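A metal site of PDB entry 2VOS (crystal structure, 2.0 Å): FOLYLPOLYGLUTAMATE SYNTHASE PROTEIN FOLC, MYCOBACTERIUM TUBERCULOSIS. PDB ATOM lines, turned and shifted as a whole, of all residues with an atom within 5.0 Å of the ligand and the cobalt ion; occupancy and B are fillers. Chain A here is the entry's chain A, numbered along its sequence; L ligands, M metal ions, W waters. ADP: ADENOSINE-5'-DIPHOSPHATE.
An oxygen (O1B) of the ligand sits close to the backbone NH (N) of Thr 76 (2.7 Å). N of Ser 77 is in hydrogen-bond range of O2A of the ligand. The side-chain hydroxyl of Ser 77 is in hydrogen-bond range of an oxygen (O2A) of the ligand (2.8 Å). An oxygen (O3B) of the ligand is in hydrogen-bond range of the backbone NH (N) of Lys 75 (2.8 Å). The side-chain amino group (NZ) of Lys 75 is in salt-bridge range of an oxygen (O3B) of the ligand (2.8 Å). NH2 of Arg 338 lies within salt-bridge range of O1A of the ligand (2.8 Å). OD2 of Asp 351 sits at hydrogen-bond distance from O2' of the ligand, at 2.9 Å. The backbone NH (N) of Gly 74 sits at hydrogen-bond distance from an oxygen (O3A) of the ligand (2.9 Å). OD1 of Asn 301 is in hydrogen-bond range of N6 of the ligand (3.0 Å). ND2 of Asn 73 is in hydrogen-bond range of O4' of the ligand, at 3.2 Å. O of Gly 358 is in hydrogen-bond range of O2' of the ligand (3.4 Å). An oxygen (O3') of the ligand is in hydrogen-bond range of the backbone NH (N) of Ala 352 (3.5 Å).
The side-chain amide nitrogen of Gln 298 lies within hydrogen-bond range of the side-chain hydroxyl of Ser 77. The side-chain hydroxyl (OG) of Ser 335 sits at hydrogen-bond distance from the side-chain hydroxyl (OG) of Ser 77, 2.9 Å away. The backbone carbonyl oxygen of Gly 71 sits at hydrogen-bond distance from the side-chain amino group of Lys 75, 3.0 Å away. The side-chain amide oxygen (OE1) of Gln 298 is in hydrogen-bond range of the side-chain amide nitrogen (ND2) of Asn 301 (2.9 Å). N of Asn 73 sits at hydrogen-bond distance from O of Pro 196 (3.2 Å). N of Thr 72 sits at hydrogen-bond distance from O of Pro 196 (3.0 Å). O of Ala 352 lies within hydrogen-bond range of ND1 of His 354. O of Gly 337 is in hydrogen-bond range of N of Ala 352 (2.9 Å).
O of Thr 72 sits close to O3B of the ligand. His 297 touches the ligand (CB to C6, 3.6 Å). Ala 353 touches the ligand (N to O3', 3.5 Å). O of Ala 357 touches C2 of the ligand (3.9 Å). Ala 361 touches the ligand (CB to N3, 3.6 Å). Hydrophobic or aromatic side chains that line the ligand: His 297, Ala 352, Ala 353 and Ala 361. Within 4 Å of the ligand: Thr 72, Asn 73, Gly 74, Lys 75, Thr 76, Ser 77, Glu 174, His 297, Asn 301, Arg 338, Asp 351, Ala 352, Ala 353, Ala 357, Gly 358 and Ala 361. The nearest printed residue that does not touch the ligand is Pro 196 (4.04 Å).
Merely in contact with the cobalt ion: Pro 99 (3.97 Å). Within 4 Å of the cobalt ion: Thr 76, Ser 98, Pro 99 and Glu 174.
The cobalt ion is bound by O1B of the ligand, water W1, water W7, OE2 of Glu 174, OG1 of Thr 76 and O of Ser 98.
Water W1 lies within hydrogen-bond range of an oxygen (O1A) of the ligand (2.8 Å) and the guanidinium group of Arg 338 (2.9 Å). Water W6 bridges O of Thr 72 (2.7 Å) and O2B of the ligand (2.8 Å). Water W3 lies within hydrogen-bond range of N of His 354 (2.9 Å), ND2 of Asn 73 (3.1 Å) and O4' of the ligand (3.5 Å).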
ATOM      1  N   GLY A  71      25.099 -23.829  -9.464  1.00  0.00           N
ATOM      2  CA  GLY A  71      26.014 -22.696  -9.522  1.00  0.00           C
ATOM      3  C   GLY A  71      25.252 -21.472  -9.111  1.00  0.00           C
ATOM      4  O   GLY A  71      24.075 -21.578  -8.741  1.00  0.00           O
ATOM      5  N   THR A  72      25.874 -20.292  -9.197  1.00  0.00           N
ATOM      6  CA  THR A  72      25.196 -19.088  -8.780  1.00  0.00           C
ATOM      7  C   THR A  72      24.662 -18.293  -9.926  1.00  0.00           C
ATOM      8  O   THR A  72      23.549 -17.766  -9.825  1.00  0.00           O
ATOM      9  CB  THR A  72      26.131 -18.155  -7.959  1.00  0.00           C
ATOM     10  OG1 THR A  72      26.600 -18.919  -6.825  1.00  0.00           O
ATOM     11  CG2 THR A  72      25.304 -16.996  -7.422  1.00  0.00           C
ATOM     12  N   ASN A  73      25.446 -18.101 -10.970  1.00  0.00           N
ATOM     13  CA  ASN A  73      24.943 -17.347 -12.110  1.00  0.00           C
ATOM     14  C   ASN A  73      25.100 -18.208 -13.406  1.00  0.00           C
ATOM     15  O   ASN A  73      26.053 -18.944 -13.533  1.00  0.00           O
ATOM     16  CB  ASN A  73      25.740 -16.074 -12.315  1.00  0.00           C
ATOM     17  CG  ASN A  73      25.377 -14.968 -11.319  1.00  0.00           C
ATOM     18  OD1 ASN A  73      26.057 -14.822 -10.325  1.00  0.00           O
ATOM     19  ND2 ASN A  73      24.316 -14.155 -11.616  1.00  0.00           N
ATOM     20  N   GLY A  74      24.155 -18.059 -14.330  1.00  0.00           N
ATOM     21  CA  GLY A  74      24.193 -18.737 -15.620  1.00  0.00           C
ATOM     22  C   GLY A  74      23.538 -20.119 -15.590  1.00  0.00           C
ATOM     23  O   GLY A  74      23.576 -20.816 -16.623  1.00  0.00           O
ATOM     24  N   LYS A  75      22.955 -20.563 -14.484  1.00  0.00           N
ATOM     25  CA  LYS A  75      22.388 -21.934 -14.516  1.00  0.00           C
ATOM     26  C   LYS A  75      21.327 -22.064 -15.608  1.00  0.00           C
ATOM     27  O   LYS A  75      21.340 -23.021 -16.389  1.00  0.00           O
ATOM     28  CB  LYS A  75      21.729 -22.435 -13.203  1.00  0.00           C
ATOM     29  CG  LYS A  75      22.689 -22.547 -11.940  1.00  0.00           C
ATOM     30  CD  LYS A  75      21.909 -23.069 -10.735  1.00  0.00           C
ATOM     31  CE  LYS A  75      20.882 -22.020 -10.213  1.00  0.00           C
ATOM     32  NZ  LYS A  75      21.505 -20.653  -9.992  1.00  0.00           N
ATOM     33  N   THR A  76      20.331 -21.185 -15.561  1.00  0.00           N
ATOM     34  CA  THR A  76      19.218 -21.261 -16.533  1.00  0.00           C
ATOM     35  C   THR A  76      19.743 -21.089 -17.963  1.00  0.00           C
ATOM     36  O   THR A  76      19.340 -21.827 -18.876  1.00  0.00           O
ATOM     37  CB  THR A  76      18.097 -20.224 -16.216  1.00  0.00           C
ATOM     38  OG1 THR A  76      17.432 -20.710 -15.057  1.00  0.00           O
ATOM     39  CG2 THR A  76      17.048 -20.233 -17.378  1.00  0.00           C
ATOM     40  N   SER A  77      20.593 -20.096 -18.161  1.00  0.00           N
ATOM     41  CA  SER A  77      21.103 -19.887 -19.520  1.00  0.00           C
ATOM     42  C   SER A  77      21.895 -21.130 -20.021  1.00  0.00           C
ATOM     43  O   SER A  77      21.763 -21.557 -21.186  1.00  0.00           O
ATOM     44  CB  SER A  77      22.042 -18.681 -19.538  1.00  0.00           C
ATOM     45  OG  SER A  77      21.348 -17.454 -19.438  1.00  0.00           O
ATOM     46  N   SER A  98      14.364 -23.027 -13.306  1.00  0.00           N
ATOM     47  CA  SER A  98      13.750 -22.206 -12.292  1.00  0.00           C
ATOM     48  C   SER A  98      14.617 -20.953 -12.068  1.00  0.00           C
ATOM     49  O   SER A  98      15.800 -20.862 -12.511  1.00  0.00           O
ATOM     50  CB  SER A  98      13.512 -22.975 -10.988  1.00  0.00           C
ATOM     51  OG  SER A  98      14.763 -23.466 -10.564  1.00  0.00           O
ATOM     52  N   PRO A  99      13.967 -19.911 -11.506  1.00  0.00           N
ATOM     53  CA  PRO A  99      12.519 -19.858 -11.314  1.00  0.00           C
ATOM     54  C   PRO A  99      11.832 -19.630 -12.688  1.00  0.00           C
ATOM     55  O   PRO A  99      12.527 -19.463 -13.670  1.00  0.00           O
ATOM     56  CB  PRO A  99      12.302 -18.622 -10.394  1.00  0.00           C
ATOM     57  CG  PRO A  99      13.649 -17.973 -10.219  1.00  0.00           C
ATOM     58  CD  PRO A  99      14.676 -18.683 -11.100  1.00  0.00           C
ATOM     59  N   GLU A 174      18.010 -28.198 -13.861  1.00  0.00           N
ATOM     60  CA  GLU A 174      18.632 -27.133 -13.100  1.00  0.00           C
ATOM     61  C   GLU A 174      18.275 -27.286 -11.606  1.00  0.00           C
ATOM     62  O   GLU A 174      17.122 -27.491 -11.261  1.00  0.00           O
ATOM     63  CB  GLU A 174      18.115 -25.777 -13.586  1.00  0.00           C
ATOM     64  CG  GLU A 174      18.531 -24.618 -12.749  1.00  0.00           C
ATOM     65  CD  GLU A 174      18.029 -23.264 -13.304  1.00  0.00           C
ATOM     66  OE1 GLU A 174      17.276 -23.192 -14.300  1.00  0.00           O
ATOM     67  OE2 GLU A 174      18.410 -22.244 -12.711  1.00  0.00           O
ATOM     68  N   PRO A 196      29.578 -20.493 -12.512  1.00  0.00           N
ATOM     69  CA  PRO A 196      30.303 -19.646 -11.546  1.00  0.00           C
ATOM     70  C   PRO A 196      29.552 -19.447 -10.266  1.00  0.00           C
ATOM     71  O   PRO A 196      28.376 -19.143 -10.267  1.00  0.00           O
ATOM     72  CB  PRO A 196      30.465 -18.310 -12.281  1.00  0.00           C
ATOM     73  CG  PRO A 196      30.600 -18.833 -13.827  1.00  0.00           C
ATOM     74  CD  PRO A 196      29.434 -19.835 -13.826  1.00  0.00           C
ATOM     75  N   HIS A 297      29.727 -12.786 -20.460  1.00  0.00           N
ATOM     76  CA  HIS A 297      29.336 -13.913 -19.609  1.00  0.00           C
ATOM     77  C   HIS A 297      28.619 -15.009 -20.382  1.00  0.00           C
ATOM     78  O   HIS A 297      28.745 -16.206 -20.032  1.00  0.00           O
ATOM     79  CB  HIS A 297      28.422 -13.482 -18.474  1.00  0.00           C
ATOM     80  CG  HIS A 297      27.192 -12.724 -18.918  1.00  0.00           C
ATOM     81  ND1 HIS A 297      27.269 -11.440 -19.420  1.00  0.00           N
ATOM     82  CD2 HIS A 297      25.868 -13.013 -18.815  1.00  0.00           C
ATOM     83  CE1 HIS A 297      26.043 -11.012 -19.703  1.00  0.00           C
ATOM     84  NE2 HIS A 297      25.176 -11.925 -19.282  1.00  0.00           N
ATOM     85  N   GLN A 298      27.843 -14.635 -21.403  1.00  0.00           N
ATOM     86  CA  GLN A 298      27.189 -15.678 -22.202  1.00  0.00           C
ATOM     87  C   GLN A 298      28.202 -16.505 -23.061  1.00  0.00           C
ATOM     88  O   GLN A 298      27.949 -17.633 -23.389  1.00  0.00           O
ATOM     89  CB  GLN A 298      26.032 -15.118 -23.047  1.00  0.00           C
ATOM     90  CG  GLN A 298      24.898 -14.521 -22.153  1.00  0.00           C
ATOM     91  CD  GLN A 298      24.104 -15.594 -21.417  1.00  0.00           C
ATOM     92  OE1 GLN A 298      24.443 -16.771 -21.449  1.00  0.00           O
ATOM     93  NE2 GLN A 298      22.999 -15.199 -20.803  1.00  0.00           N
ATOM     94  N   ASN A 301      29.215 -19.125 -20.530  1.00  0.00           N
ATOM     95  CA  ASN A 301      28.111 -20.074 -20.394  1.00  0.00           C
ATOM     96  C   ASN A 301      28.085 -20.990 -21.639  1.00  0.00           C
ATOM     97  O   ASN A 301      27.912 -22.185 -21.493  1.00  0.00           O
ATOM     98  CB  ASN A 301      26.738 -19.374 -20.303  1.00  0.00           C
ATOM     99  CG  ASN A 301      26.589 -18.571 -19.007  1.00  0.00           C
ATOM    100  OD1 ASN A 301      27.358 -18.794 -18.060  1.00  0.00           O
ATOM    101  ND2 ASN A 301      25.593 -17.691 -18.942  1.00  0.00           N
ATOM    102  N   SER A 335      17.433 -16.977 -24.316  1.00  0.00           N
ATOM    103  CA  SER A 335      17.431 -16.954 -22.838  1.00  0.00           C
ATOM    104  C   SER A 335      16.542 -15.754 -22.412  1.00  0.00           C
ATOM    105  O   SER A 335      17.024 -14.662 -22.199  1.00  0.00           O
ATOM    106  CB  SER A 335      18.847 -16.853 -22.281  1.00  0.00           C
ATOM    107  OG  SER A 335      18.830 -17.112 -20.856  1.00  0.00           O
ATOM    108  N   GLY A 337      14.469 -12.926 -20.808  1.00  0.00           N
ATOM    109  CA  GLY A 337      14.736 -12.134 -19.604  1.00  0.00           C
ATOM    110  C   GLY A 337      16.184 -12.055 -19.234  1.00  0.00           C
ATOM    111  O   GLY A 337      16.468 -11.571 -18.144  1.00  0.00           O
ATOM    112  N   ARG A 338      17.129 -12.527 -20.073  1.00  0.00           N
ATOM    113  CA  ARG A 338      18.582 -12.254 -19.838  1.00  0.00           C
ATOM    114  C   ARG A 338      19.101 -11.311 -20.933  1.00  0.00           C
ATOM    115  O   ARG A 338      19.310 -11.695 -22.106  1.00  0.00           O
ATOM    116  CB  ARG A 338      19.426 -13.548 -19.810  1.00  0.00           C
ATOM    117  CG  ARG A 338      19.264 -14.354 -18.476  1.00  0.00           C
ATOM    118  CD  ARG A 338      17.802 -14.643 -18.198  1.00  0.00           C
ATOM    119  NE  ARG A 338      17.572 -15.583 -17.098  1.00  0.00           N
ATOM    120  CZ  ARG A 338      16.362 -16.026 -16.702  1.00  0.00           C
ATOM    121  NH1 ARG A 338      15.232 -15.625 -17.287  1.00  0.00           N
ATOM    122  NH2 ARG A 338      16.267 -16.866 -15.699  1.00  0.00           N
ATOM    123  N   LEU A 339      19.227 -10.037 -20.543  1.00  0.00           N
ATOM    124  CA  LEU A 339      19.572  -8.967 -21.455  1.00  0.00           C
ATOM    125  C   LEU A 339      18.788  -9.084 -22.752  1.00  0.00           C
ATOM    126  O   LEU A 339      19.367  -9.120 -23.863  1.00  0.00           O
ATOM    127  CB  LEU A 339      21.063  -9.014 -21.750  1.00  0.00           C
ATOM    128  CG  LEU A 339      22.042  -7.850 -21.466  1.00  0.00           C
ATOM    129  CD1 LEU A 339      21.459  -6.540 -21.080  1.00  0.00           C
ATOM    130  CD2 LEU A 339      23.169  -8.373 -20.580  1.00  0.00           C
ATOM    131  N   ASP A 351      16.290  -7.732 -17.789  1.00  0.00           N
ATOM    132  CA  ASP A 351      17.353  -8.570 -17.303  1.00  0.00           C
ATOM    133  C   ASP A 351      17.065  -9.027 -15.876  1.00  0.00           C
ATOM    134  O   ASP A 351      16.750  -8.211 -15.000  1.00  0.00           O
ATOM    135  CB  ASP A 351      18.716  -7.885 -17.404  1.00  0.00           C
ATOM    136  CG  ASP A 351      19.864  -8.897 -17.188  1.00  0.00           C
ATOM    137  OD1 ASP A 351      20.238  -9.651 -18.085  1.00  0.00           O
ATOM    138  OD2 ASP A 351      20.338  -9.012 -16.083  1.00  0.00           O
ATOM    139  N   ALA A 352      17.197 -10.336 -15.642  1.00  0.00           N
ATOM    140  CA  ALA A 352      16.880 -10.947 -14.369  1.00  0.00           C
ATOM    141  C   ALA A 352      17.969 -10.678 -13.284  1.00  0.00           C
ATOM    142  O   ALA A 352      17.825 -11.191 -12.159  1.00  0.00           O
ATOM    143  CB  ALA A 352      16.729 -12.462 -14.538  1.00  0.00           C
ATOM    144  N   ALA A 353      19.038  -9.927 -13.588  1.00  0.00           N
ATOM    145  CA  ALA A 353      20.122  -9.740 -12.617  1.00  0.00           C
ATOM    146  C   ALA A 353      19.578  -9.453 -11.222  1.00  0.00           C
ATOM    147  O   ALA A 353      18.751  -8.556 -11.030  1.00  0.00           O
ATOM    148  CB  ALA A 353      21.047  -8.614 -13.046  1.00  0.00           C
ATOM    149  N   HIS A 354      20.053 -10.211 -10.239  1.00  0.00           N
ATOM    150  CA  HIS A 354      19.559 -10.084  -8.872  1.00  0.00           C
ATOM    151  C   HIS A 354      20.695 -10.403  -7.866  1.00  0.00           C
ATOM    152  O   HIS A 354      20.427 -10.778  -6.684  1.00  0.00           O
ATOM    153  CB  HIS A 354      18.361 -10.987  -8.627  1.00  0.00           C
ATOM    154  CG  HIS A 354      18.661 -12.428  -8.844  1.00  0.00           C
ATOM    155  ND1 HIS A 354      18.355 -13.068 -10.018  1.00  0.00           N
ATOM    156  CD2 HIS A 354      19.270 -13.331  -8.062  1.00  0.00           C
ATOM    157  CE1 HIS A 354      18.726 -14.326  -9.936  1.00  0.00           C
ATOM    158  NE2 HIS A 354      19.289 -14.511  -8.757  1.00  0.00           N
ATOM    159  N   ALA A 357      27.413 -10.175  -8.966  1.00  0.00           N
ATOM    160  CA  ALA A 357      27.992 -10.738 -10.188  1.00  0.00           C
ATOM    161  C   ALA A 357      27.101 -10.535 -11.451  1.00  0.00           C
ATOM    162  O   ALA A 357      27.620 -10.141 -12.497  1.00  0.00           O
ATOM    163  CB  ALA A 357      28.342 -12.208 -10.034  1.00  0.00           C
ATOM    164  N   GLY A 358      25.787 -10.812 -11.360  1.00  0.00           N
ATOM    165  CA  GLY A 358      24.911 -10.607 -12.496  1.00  0.00           C
ATOM    166  C   GLY A 358      24.743  -9.116 -12.848  1.00  0.00           C
ATOM    167  O   GLY A 358      24.686  -8.768 -14.040  1.00  0.00           O
ATOM    168  N   ALA A 361      27.721  -8.107 -14.681  1.00  0.00           N
ATOM    169  CA  ALA A 361      27.760  -8.637 -16.073  1.00  0.00           C
ATOM    170  C   ALA A 361      26.854  -7.773 -16.967  1.00  0.00           C
ATOM    171  O   ALA A 361      27.232  -7.387 -18.093  1.00  0.00           O
ATOM    172  CB  ALA A 361      27.309 -10.068 -16.111  1.00  0.00           C
ATOM    173  N   LEU A 362      25.680  -7.433 -16.432  1.00  0.00           N
ATOM    174  CA  LEU A 362      24.759  -6.552 -17.079  1.00  0.00           C
ATOM    175  C   LEU A 362      25.391  -5.172 -17.388  1.00  0.00           C
ATOM    176  O   LEU A 362      25.295  -4.670 -18.533  1.00  0.00           O
ATOM    177  CB  LEU A 362      23.488  -6.389 -16.211  1.00  0.00           C
ATOM    178  CG  LEU A 362      22.442  -5.367 -16.622  1.00  0.00           C
ATOM    179  CD1 LEU A 362      21.949  -5.544 -18.116  1.00  0.00           C
ATOM    180  CD2 LEU A 362      21.211  -5.378 -15.625  1.00  0.00           C
HETATM  181  PB  ADP L   1      20.661 -18.622 -12.806  1.00  0.00           P
HETATM  182  O1B ADP L   1      19.737 -19.638 -13.421  1.00  0.00           O
HETATM  183  O2B ADP L   1      19.970 -17.688 -11.846  1.00  0.00           O
HETATM  184  O3B ADP L   1      21.973 -19.134 -12.284  1.00  0.00           O
HETATM  185  PA  ADP L   1      20.515 -17.148 -15.373  1.00  0.00           P
HETATM  186  O1A ADP L   1      19.015 -17.079 -15.162  1.00  0.00           O
HETATM  187  O2A ADP L   1      21.206 -17.576 -16.662  1.00  0.00           O
HETATM  188  O3A ADP L   1      21.247 -17.715 -14.022  1.00  0.00           O
HETATM  189  O5' ADP L   1      20.954 -15.592 -15.243  1.00  0.00           O
HETATM  190  C5' ADP L   1      20.453 -14.675 -14.251  1.00  0.00           C
HETATM  191  C4' ADP L   1      21.211 -13.343 -14.498  1.00  0.00           C
HETATM  192  O4' ADP L   1      22.624 -13.553 -14.206  1.00  0.00           O
HETATM  193  C3' ADP L   1      21.244 -12.896 -15.958  1.00  0.00           C
HETATM  194  O3' ADP L   1      20.262 -11.918 -16.210  1.00  0.00           O
HETATM  195  C2' ADP L   1      22.565 -12.219 -16.216  1.00  0.00           C
HETATM  196  O2' ADP L   1      22.463 -10.873 -15.628  1.00  0.00           O
HETATM  197  C1' ADP L   1      23.452 -12.905 -15.218  1.00  0.00           C
HETATM  198  N9  ADP L   1      24.300 -14.021 -15.729  1.00  0.00           N
HETATM  199  C8  ADP L   1      23.982 -15.160 -16.430  1.00  0.00           C
HETATM  200  N7  ADP L   1      25.103 -15.912 -16.624  1.00  0.00           N
HETATM  201  C5  ADP L   1      26.112 -15.297 -15.942  1.00  0.00           C
HETATM  202  C6  ADP L   1      27.531 -15.561 -15.679  1.00  0.00           C
HETATM  203  N6  ADP L   1      28.141 -16.657 -16.179  1.00  0.00           N
HETATM  204  N1  ADP L   1      28.191 -14.629 -14.979  1.00  0.00           N
HETATM  205  C2  ADP L   1      27.680 -13.477 -14.487  1.00  0.00           C
HETATM  206  N3  ADP L   1      26.360 -13.174 -14.645  1.00  0.00           N
HETATM  207  C4  ADP L   1      25.585 -14.050 -15.373  1.00  0.00           C
HETATM  208 CO    CO M   1      17.843 -20.179 -12.973  1.00  0.00          CO
HETATM  209 MG    MG M   2      20.062 -16.328  -8.215  1.00  0.00          MG
HETATM  210  O   HOH W   1      17.223 -18.193 -13.323  1.00  0.00           O
HETATM  211  O   HOH W   2      30.683 -14.849 -13.678  1.00  0.00           O
HETATM  212  O   HOH W   3      21.762 -12.439 -11.053  1.00  0.00           O
HETATM  213  O   HOH W   4      31.329 -16.165 -16.478  1.00  0.00           O
HETATM  214  O   HOH W   5      17.670 -16.977 -11.289  1.00  0.00           O
HETATM  215  O   HOH W   6      21.419 -16.062 -10.126  1.00  0.00           O
HETATM  216  O   HOH W   7      18.041 -19.802 -10.860  1.00  0.00           O
